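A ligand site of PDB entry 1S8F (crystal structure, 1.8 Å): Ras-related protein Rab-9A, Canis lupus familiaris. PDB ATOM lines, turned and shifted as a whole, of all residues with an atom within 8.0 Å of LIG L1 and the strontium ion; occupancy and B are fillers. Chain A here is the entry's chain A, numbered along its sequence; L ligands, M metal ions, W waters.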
ATOM      1  N   GLY A  16     -21.512   5.745  -2.581  1.00  0.00           N
ATOM      2  CA  GLY A  16     -21.368   5.239  -3.941  1.00  0.00           C
ATOM      3  C   GLY A  16     -20.996   3.773  -3.839  1.00  0.00           C
ATOM      4  O   GLY A  16     -20.687   3.293  -2.749  1.00  0.00           O
ATOM      5  N   ASP A  17     -21.020   3.052  -4.953  1.00  0.00           N
ATOM      6  CA  ASP A  17     -20.687   1.639  -4.925  1.00  0.00           C
ATOM      7  C   ASP A  17     -19.340   1.344  -4.288  1.00  0.00           C
ATOM      8  O   ASP A  17     -18.372   2.105  -4.254  1.00  0.00           O
ATOM      9  CB  ASP A  17     -20.665   1.063  -6.360  1.00  0.00           C
ATOM     10  CG  ASP A  17     -22.018   0.990  -7.017  1.00  0.00           C
ATOM     11  OD1 ASP A  17     -23.058   1.352  -6.422  1.00  0.00           O
ATOM     12  OD2 ASP A  17     -22.074   0.559  -8.203  1.00  0.00           O
ATOM     13  N   GLY A  18     -19.247   0.102  -3.792  1.00  0.00           N
ATOM     14  CA  GLY A  18     -17.977  -0.369  -3.249  1.00  0.00           C
ATOM     15  C   GLY A  18     -16.925  -0.383  -4.343  1.00  0.00           C
ATOM     16  O   GLY A  18     -17.146  -0.794  -5.486  1.00  0.00           O
ATOM     17  N   GLY A  19     -15.724   0.079  -4.031  1.00  0.00           N
ATOM     18  CA  GLY A  19     -14.639   0.096  -4.972  1.00  0.00           C
ATOM     19  C   GLY A  19     -14.436   1.368  -5.747  1.00  0.00           C
ATOM     20  O   GLY A  19     -13.387   1.529  -6.375  1.00  0.00           O
ATOM     21  N   VAL A  20     -15.374   2.305  -5.746  1.00  0.00           N
ATOM     22  CA  VAL A  20     -15.216   3.501  -6.579  1.00  0.00           C
ATOM     23  C   VAL A  20     -14.136   4.469  -6.101  1.00  0.00           C
ATOM     24  O   VAL A  20     -13.695   5.337  -6.869  1.00  0.00           O
ATOM     25  CB  VAL A  20     -16.526   4.291  -6.728  1.00  0.00           C
ATOM     26  CG1 VAL A  20     -17.633   3.436  -7.328  1.00  0.00           C
ATOM     27  CG2 VAL A  20     -16.945   4.855  -5.371  1.00  0.00           C
ATOM     28  N   GLY A  21     -13.706   4.302  -4.848  1.00  0.00           N
ATOM     29  CA  GLY A  21     -12.602   5.024  -4.274  1.00  0.00           C
ATOM     30  C   GLY A  21     -12.897   5.985  -3.158  1.00  0.00           C
ATOM     31  O   GLY A  21     -12.116   6.911  -2.939  1.00  0.00           O
ATOM     32  N   LYS A  22     -13.964   5.779  -2.403  1.00  0.00           N
ATOM     33  CA  LYS A  22     -14.370   6.710  -1.329  1.00  0.00           C
ATOM     34  C   LYS A  22     -13.325   6.798  -0.221  1.00  0.00           C
ATOM     35  O   LYS A  22     -12.936   7.916   0.151  1.00  0.00           O
ATOM     36  CB  LYS A  22     -15.723   6.259  -0.807  1.00  0.00           C
ATOM     37  CG  LYS A  22     -16.840   6.184  -1.829  1.00  0.00           C
ATOM     38  CD  LYS A  22     -18.132   5.750  -1.157  1.00  0.00           C
ATOM     39  CE  LYS A  22     -18.057   4.319  -0.672  1.00  0.00           C
ATOM     40  NZ  LYS A  22     -17.811   3.337  -1.743  1.00  0.00           N
ATOM     41  N   SER A  23     -12.883   5.665   0.301  1.00  0.00           N
ATOM     42  CA  SER A  23     -11.896   5.599   1.380  1.00  0.00           C
ATOM     43  C   SER A  23     -10.625   6.318   0.937  1.00  0.00           C
ATOM     44  O   SER A  23     -10.028   7.140   1.635  1.00  0.00           O
ATOM     45  CB  SER A  23     -11.638   4.153   1.754  1.00  0.00           C
ATOM     46  OG  SER A  23     -12.651   3.537   2.515  1.00  0.00           O
ATOM     47  N   SER A  24     -10.197   6.035  -0.300  1.00  0.00           N
ATOM     48  CA  SER A  24      -9.010   6.657  -0.851  1.00  0.00           C
ATOM     49  C   SER A  24      -9.160   8.145  -1.069  1.00  0.00           C
ATOM     50  O   SER A  24      -8.191   8.879  -0.822  1.00  0.00           O
ATOM     51  CB  SER A  24      -8.662   5.993  -2.194  1.00  0.00           C
ATOM     52  OG  SER A  24      -8.537   4.593  -1.987  1.00  0.00           O
ATOM     53  N   MET A  26     -10.997  10.138   0.694  1.00  0.00           N
ATOM     54  CA  MET A  26     -10.973  10.713   2.046  1.00  0.00           C
ATOM     55  C   MET A  26      -9.527  10.815   2.521  1.00  0.00           C
ATOM     56  O   MET A  26      -9.011  11.824   2.991  1.00  0.00           O
ATOM     57  CB  MET A  26     -11.774   9.859   3.027  1.00  0.00           C
ATOM     58  CG  MET A  26     -13.277   9.873   2.812  1.00  0.00           C
ATOM     59  SD  MET A  26     -14.018   8.442   3.601  1.00  0.00           S
ATOM     60  CE  MET A  26     -13.723   8.768   5.339  1.00  0.00           C
ATOM     61  N   LEU A  38      -5.894   0.085   2.261  1.00  0.00           N
ATOM     62  CA  LEU A  38      -6.729   0.681   3.307  1.00  0.00           C
ATOM     63  C   LEU A  38      -7.542  -0.447   3.927  1.00  0.00           C
ATOM     64  O   LEU A  38      -7.807  -1.442   3.243  1.00  0.00           O
ATOM     65  CB  LEU A  38      -7.615   1.809   2.769  1.00  0.00           C
ATOM     66  CG  LEU A  38      -6.870   3.087   2.353  1.00  0.00           C
ATOM     67  CD1 LEU A  38      -7.787   3.996   1.531  1.00  0.00           C
ATOM     68  CD2 LEU A  38      -6.316   3.810   3.569  1.00  0.00           C
ATOM     69  N   PHE A  39      -7.914  -0.263   5.193  1.00  0.00           N
ATOM     70  CA  PHE A  39      -8.782  -1.269   5.790  1.00  0.00           C
ATOM     71  C   PHE A  39     -10.105  -1.322   5.018  1.00  0.00           C
ATOM     72  O   PHE A  39     -10.548  -0.303   4.497  1.00  0.00           O
ATOM     73  CB  PHE A  39      -9.087  -0.949   7.233  1.00  0.00           C
ATOM     74  CG  PHE A  39      -8.003  -1.167   8.258  1.00  0.00           C
ATOM     75  CD1 PHE A  39      -6.966  -0.260   8.351  1.00  0.00           C
ATOM     76  CD2 PHE A  39      -8.033  -2.252   9.125  1.00  0.00           C
ATOM     77  CE1 PHE A  39      -5.975  -0.422   9.302  1.00  0.00           C
ATOM     78  CE2 PHE A  39      -7.050  -2.408  10.086  1.00  0.00           C
ATOM     79  CZ  PHE A  39      -6.029  -1.485  10.169  1.00  0.00           C
ATOM     80  N   HIS A  40     -10.662  -2.517   4.969  1.00  0.00           N
ATOM     81  CA  HIS A  40     -11.998  -2.806   4.496  1.00  0.00           C
ATOM     82  C   HIS A  40     -12.906  -2.716   5.721  1.00  0.00           C
ATOM     83  O   HIS A  40     -12.743  -3.495   6.652  1.00  0.00           O
ATOM     84  CB  HIS A  40     -12.084  -4.165   3.824  1.00  0.00           C
ATOM     85  CG  HIS A  40     -11.188  -4.172   2.627  1.00  0.00           C
ATOM     86  ND1 HIS A  40     -11.321  -3.322   1.561  1.00  0.00           N
ATOM     87  CD2 HIS A  40     -10.128  -4.975   2.343  1.00  0.00           C
ATOM     88  CE1 HIS A  40     -10.372  -3.592   0.675  1.00  0.00           C
ATOM     89  NE2 HIS A  40      -9.644  -4.584   1.117  1.00  0.00           N
ATOM     90  N   THR A  41     -13.809  -1.742   5.676  1.00  0.00           N
ATOM     91  CA  THR A  41     -14.682  -1.566   6.824  1.00  0.00           C
ATOM     92  C   THR A  41     -16.095  -2.040   6.488  1.00  0.00           C
ATOM     93  O   THR A  41     -16.781  -1.531   5.600  1.00  0.00           O
ATOM     94  CB  THR A  41     -14.735  -0.130   7.345  1.00  0.00           C
ATOM     95  OG1 THR A  41     -13.421   0.248   7.816  1.00  0.00           O
ATOM     96  CG2 THR A  41     -15.683  -0.017   8.512  1.00  0.00           C
ATOM     97  N   ILE A  42     -16.518  -3.031   7.256  1.00  0.00           N
ATOM     98  CA  ILE A  42     -17.910  -3.439   7.288  1.00  0.00           C
ATOM     99  C   ILE A  42     -18.615  -2.561   8.334  1.00  0.00           C
ATOM    100  O   ILE A  42     -18.618  -2.840   9.536  1.00  0.00           O
ATOM    101  CB  ILE A  42     -18.054  -4.940   7.542  1.00  0.00           C
ATOM    102  CG1 ILE A  42     -17.334  -5.812   6.503  1.00  0.00           C
ATOM    103  CG2 ILE A  42     -19.528  -5.299   7.614  1.00  0.00           C
ATOM    104  CD1 ILE A  42     -17.348  -7.290   6.807  1.00  0.00           C
ATOM    105  N   GLY A  43     -19.160  -1.475   7.802  1.00  0.00           N
ATOM    106  CA  GLY A  43     -19.813  -0.416   8.540  1.00  0.00           C
ATOM    107  C   GLY A  43     -19.499   0.925   7.936  1.00  0.00           C
ATOM    108  O   GLY A  43     -19.731   1.155   6.742  1.00  0.00           O
ATOM    109  N   GLU A  45     -16.905   4.787   8.335  1.00  0.00           N
ATOM    110  CA  GLU A  45     -15.574   5.283   8.653  1.00  0.00           C
ATOM    111  C   GLU A  45     -15.618   6.802   8.625  1.00  0.00           C
ATOM    112  O   GLU A  45     -16.413   7.354   7.867  1.00  0.00           O
ATOM    113  CB  GLU A  45     -14.509   4.896   7.630  1.00  0.00           C
ATOM    114  CG  GLU A  45     -14.756   3.656   6.802  1.00  0.00           C
ATOM    115  CD  GLU A  45     -13.707   3.403   5.745  1.00  0.00           C
ATOM    116  OE1 GLU A  45     -12.919   2.444   5.896  1.00  0.00           O
ATOM    117  OE2 GLU A  45     -13.718   4.181   4.781  1.00  0.00           O
ATOM    118  N   ASP A  64     -17.673   7.879   5.153  1.00  0.00           N
ATOM    119  CA  ASP A  64     -18.117   7.067   4.003  1.00  0.00           C
ATOM    120  C   ASP A  64     -18.560   5.727   4.562  1.00  0.00           C
ATOM    121  O   ASP A  64     -18.614   5.523   5.782  1.00  0.00           O
ATOM    122  CB  ASP A  64     -17.060   6.905   2.916  1.00  0.00           C
ATOM    123  CG  ASP A  64     -16.068   5.790   3.167  1.00  0.00           C
ATOM    124  OD1 ASP A  64     -15.749   5.067   2.197  1.00  0.00           O
ATOM    125  OD2 ASP A  64     -15.614   5.652   4.325  1.00  0.00           O
ATOM    126  N   THR A  65     -18.959   4.826   3.680  1.00  0.00           N
ATOM    127  CA  THR A  65     -19.614   3.607   4.127  1.00  0.00           C
ATOM    128  C   THR A  65     -19.156   2.434   3.277  1.00  0.00           C
ATOM    129  O   THR A  65     -18.636   2.681   2.197  1.00  0.00           O
ATOM    130  CB  THR A  65     -21.145   3.681   3.991  1.00  0.00           C
ATOM    131  OG1 THR A  65     -21.435   3.577   2.584  1.00  0.00           O
ATOM    132  CG2 THR A  65     -21.756   4.975   4.475  1.00  0.00           C
ATOM    133  N   ALA A  66     -19.399   1.242   3.764  1.00  0.00           N
ATOM    134  CA  ALA A  66     -19.401   0.040   2.948  1.00  0.00           C
ATOM    135  C   ALA A  66     -20.445   0.179   1.836  1.00  0.00           C
ATOM    136  O   ALA A  66     -21.545   0.661   2.088  1.00  0.00           O
ATOM    137  CB  ALA A  66     -19.729  -1.146   3.817  1.00  0.00           C
ATOM    138  N   GLY A  67     -20.180  -0.252   0.612  1.00  0.00           N
ATOM    139  CA  GLY A  67     -21.135  -0.032  -0.473  1.00  0.00           C
ATOM    140  C   GLY A  67     -22.080  -1.183  -0.747  1.00  0.00           C
ATOM    141  O   GLY A  67     -23.078  -0.982  -1.464  1.00  0.00           O
ATOM    142  N   GLN A  68     -21.824  -2.347  -0.157  1.00  0.00           N
ATOM    143  CA  GLN A  68     -22.675  -3.510  -0.439  1.00  0.00           C
ATOM    144  C   GLN A  68     -24.094  -3.345   0.059  1.00  0.00           C
ATOM    145  O   GLN A  68     -24.369  -2.879   1.154  1.00  0.00           O
ATOM    146  CB  GLN A  68     -22.093  -4.794   0.176  1.00  0.00           C
ATOM    147  CG  GLN A  68     -20.732  -5.120  -0.414  1.00  0.00           C
ATOM    148  CD  GLN A  68     -19.604  -4.554   0.436  1.00  0.00           C
ATOM    149  OE1 GLN A  68     -19.752  -3.487   1.030  1.00  0.00           O
ATOM    150  NE2 GLN A  68     -18.516  -5.305   0.448  1.00  0.00           N
ATOM    151  N   ARG A  70     -26.085  -5.537   1.179  1.00  0.00           N
ATOM    152  CA  ARG A  70     -26.380  -6.211   2.441  1.00  0.00           C
ATOM    153  C   ARG A  70     -25.893  -5.448   3.685  1.00  0.00           C
ATOM    154  O   ARG A  70     -26.332  -5.871   4.761  1.00  0.00           O
ATOM    155  CB  ARG A  70     -25.766  -7.603   2.475  1.00  0.00           C
ATOM    156  CG  ARG A  70     -24.252  -7.682   2.491  1.00  0.00           C
ATOM    157  CD  ARG A  70     -23.839  -9.123   2.737  1.00  0.00           C
ATOM    158  NE  ARG A  70     -22.441  -9.375   2.416  1.00  0.00           N
ATOM    159  CZ  ARG A  70     -21.492 -10.019   3.064  1.00  0.00           C
ATOM    160  NH1 ARG A  70     -21.741 -10.575   4.219  1.00  0.00           N
ATOM    161  NH2 ARG A  70     -20.277 -10.112   2.533  1.00  0.00           N
ATOM    162  N   PHE A  71     -25.094  -4.415   3.524  1.00  0.00           N
ATOM    163  CA  PHE A  71     -24.618  -3.691   4.737  1.00  0.00           C
ATOM    164  C   PHE A  71     -25.373  -2.391   4.939  1.00  0.00           C
ATOM    165  O   PHE A  71     -24.937  -1.549   5.720  1.00  0.00           O
ATOM    166  CB  PHE A  71     -23.118  -3.459   4.663  1.00  0.00           C
ATOM    167  CG  PHE A  71     -22.335  -4.759   4.695  1.00  0.00           C
ATOM    168  CD1 PHE A  71     -22.685  -5.817   5.502  1.00  0.00           C
ATOM    169  CD2 PHE A  71     -21.205  -4.891   3.899  1.00  0.00           C
ATOM    170  CE1 PHE A  71     -21.925  -6.972   5.489  1.00  0.00           C
ATOM    171  CE2 PHE A  71     -20.467  -6.036   3.847  1.00  0.00           C
ATOM    172  CZ  PHE A  71     -20.835  -7.102   4.639  1.00  0.00           C
HETATM  173  C1  LIG L   1     -14.396  -1.565   1.422  1.00  0.00           C
HETATM  174  O1  LIG L   1     -13.081  -1.379   1.023  1.00  0.00           O
HETATM  175  O2  LIG L   1     -15.170  -0.524   1.419  1.00  0.00           O
HETATM  176  C2  LIG L   1     -14.899  -2.922   1.832  1.00  0.00           C
HETATM  177  C3  LIG L   1     -15.857  -3.014   2.832  1.00  0.00           C
HETATM  178  C4  LIG L   1     -16.272  -4.287   3.164  1.00  0.00           C
HETATM  179  C5  LIG L   1     -15.752  -5.430   2.513  1.00  0.00           C
HETATM  180  C6  LIG L   1     -14.803  -5.317   1.531  1.00  0.00           C
HETATM  181  C7  LIG L   1     -14.382  -4.050   1.189  1.00  0.00           C
HETATM  182  P1  LG2 L   2     -14.283   2.462  -1.773  1.00  0.00           P
HETATM  183  O1  LG2 L   2     -15.243   3.226  -2.536  1.00  0.00           O
HETATM  184  O2  LG2 L   2     -14.679   1.031  -1.561  1.00  0.00           O
HETATM  185  O3  LG2 L   2     -13.893   2.949  -0.380  1.00  0.00           O
HETATM  186  O4  LG2 L   2     -12.927   2.463  -2.729  1.00  0.00           O
HETATM  187  P2  LG2 L   2     -11.450   2.314  -2.086  1.00  0.00           P
HETATM  188  O5  LG2 L   2     -11.508   1.374  -0.929  1.00  0.00           O
HETATM  189  O6  LG2 L   2     -10.828   3.645  -1.599  1.00  0.00           O
HETATM  190  O7  LG2 L   2     -10.640   1.812  -3.354  1.00  0.00           O
HETATM  191  C1  LG2 L   2     -11.034   0.687  -4.099  1.00  0.00           C
HETATM  192  C2  LG2 L   2      -9.809   0.411  -5.002  1.00  0.00           C
HETATM  193  O8  LG2 L   2      -9.680   1.498  -5.902  1.00  0.00           O
HETATM  194  C3  LG2 L   2      -8.539   0.367  -4.178  1.00  0.00           C
HETATM  195  O9  LG2 L   2      -7.707  -0.654  -4.702  1.00  0.00           O
HETATM  196  C4  LG2 L   2      -7.874   1.713  -4.412  1.00  0.00           C
HETATM  197  O10 LG2 L   2      -6.484   1.802  -4.256  1.00  0.00           O
HETATM  198  C5  LG2 L   2      -8.392   2.091  -5.781  1.00  0.00           C
HETATM  199  N1  LG2 L   2      -8.457   3.538  -5.968  1.00  0.00           N
HETATM  200  C6  LG2 L   2      -9.114   4.469  -5.204  1.00  0.00           C
HETATM  201  N2  LG2 L   2      -9.142   5.632  -5.865  1.00  0.00           N
HETATM  202  C7  LG2 L   2      -8.508   5.484  -7.059  1.00  0.00           C
HETATM  203  C8  LG2 L   2      -8.225   6.317  -8.151  1.00  0.00           C
HETATM  204  O11 LG2 L   2      -8.536   7.496  -8.242  1.00  0.00           O
HETATM  205  N3  LG2 L   2      -7.535   5.801  -9.233  1.00  0.00           N
HETATM  206  C9  LG2 L   2      -7.123   4.471  -9.261  1.00  0.00           C
HETATM  207  N4  LG2 L   2      -6.462   3.978 -10.310  1.00  0.00           N
HETATM  208  N5  LG2 L   2      -7.390   3.633  -8.202  1.00  0.00           N
HETATM  209  C10 LG2 L   2      -8.079   4.149  -7.120  1.00  0.00           C
HETATM  210 SR    SR M   1     -13.296   1.282   1.193  1.00  0.00          SR
HETATM  211  O   HOH W   1     -17.343   1.320   0.022  1.00  0.00           O
HETATM  212  O   HOH W   2     -13.649  -1.406  -2.048  1.00  0.00           O
HETATM  213  O   HOH W   3     -17.581  -1.625   0.342  1.00  0.00           O
HETATM  214  O   HOH W   4     -13.353   0.641   3.813  1.00  0.00           O
HETATM  215  O   HOH W   5     -16.325   0.547   3.787  1.00  0.00           O
HETATM  216  O   HOH W   6     -15.505   2.329   2.119  1.00  0.00           O
HETATM  217  O   HOH W   7     -11.119   0.617   1.762  1.00  0.00           O
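OG of Ser 23 lies close to OE2 of Glu 45, 2.6 Å away.
The side-chain carboxylate (OD1) of Asp 64 lies within hydrogen-bond range of the backbone NH (N) of Ser 23 (3.5 Å).
The side-chain carboxylate (OE1) of Glu 45 is in hydrogen-bond range of the side-chain hydroxyl (OG1) of Thr 41 (3.0 Å).
O6 of LG2 L2 is in hydrogen-bond range of OG of Ser 24.
The side-chain amino group (NZ) of Lys 22 is in salt-bridge range of an oxygen (O1) of LG2 L2 (2.7 Å).
An oxygen (O2) of LG2 L2 sits close to the backbone NH (N) of Gly 19 (2.8 Å).
The backbone NH (N) of Gly 21 lies within hydrogen-bond range of an oxygen (O4) of LG2 L2, 2.9 Å away.
An oxygen (O1) of LIG L1 sits close to a ring nitrogen (ND1) of His 40 (2.7 Å).
N of Ser 23 is in hydrogen-bond range of O6 of LG2 L2, 3.5 Å away.
The backbone NH (N) of Val 20 lies within hydrogen-bond range of an oxygen (O1) of LG2 L2 (3.3 Å).
O6 of LG2 L2 lies within hydrogen-bond range of N of Ser 24 (2.8 Å).
The backbone NH of Lys 22 lies within hydrogen-bond range of an oxygen (O1) of LG2 L2 (2.9 Å).
Water W6 lies within hydrogen-bond range of the side-chain carboxylate of Asp 64 and the backbone carbonyl oxygen of Thr 65.
Water W4 lies within hydrogen-bond range of OE1 of Glu 45 (2.8 Å), O of Phe 39 (3.0 Å) and N of Thr 41 (3.1 Å).
Water W5 lies within hydrogen-bond range of O of Thr 41 (2.8 Å) and N of Ala 66 (3.2 Å).
Water W3 lies within hydrogen-bond range of OE1 of Gln 68 (2.9 Å) and N of Gly 67 (3.0 Å).
Water W1 lies within hydrogen-bond range of the side-chain amino group (NZ) of Lys 22 (2.7 Å), the backbone carbonyl oxygen (O) of Thr 65 (2.9 Å) and the backbone NH (N) of Gly 67 (3.3 Å).
Water W7 binds the strontium ion, at 2.3 Å.
An oxygen (O3) of LG2 L2 binds the strontium ion, at 2.4 Å.
O2 of LIG L1 binds the strontium ion, at 2.6 Å.
The strontium ion is bound by water W6, at 2.6 Å.
The strontium ion is bound by O1 of LIG L1 (2.7 Å).
OG of Ser 23 is bound to the strontium ion, 2.7 Å away.
The strontium ion is bound by water W4, at 2.7 Å.
The strontium ion is bound by O5 of LG2 L2, 2.8 Å away.
O2 of LG2 L2 is bound to the strontium ion (3.1 Å).
The nearest printed residue that does not touch the strontium ion is Phe 39 (4.6 Å).
Merely in contact with LIG L1: Thr 41, Ile 42 and Gln 68.
Hydrophobic or aromatic side chains that line LIG L1: His 40 and Ile 42.
The nearest printed residue that does not touch LIG L1 is Ala 66 (4.4 Å).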
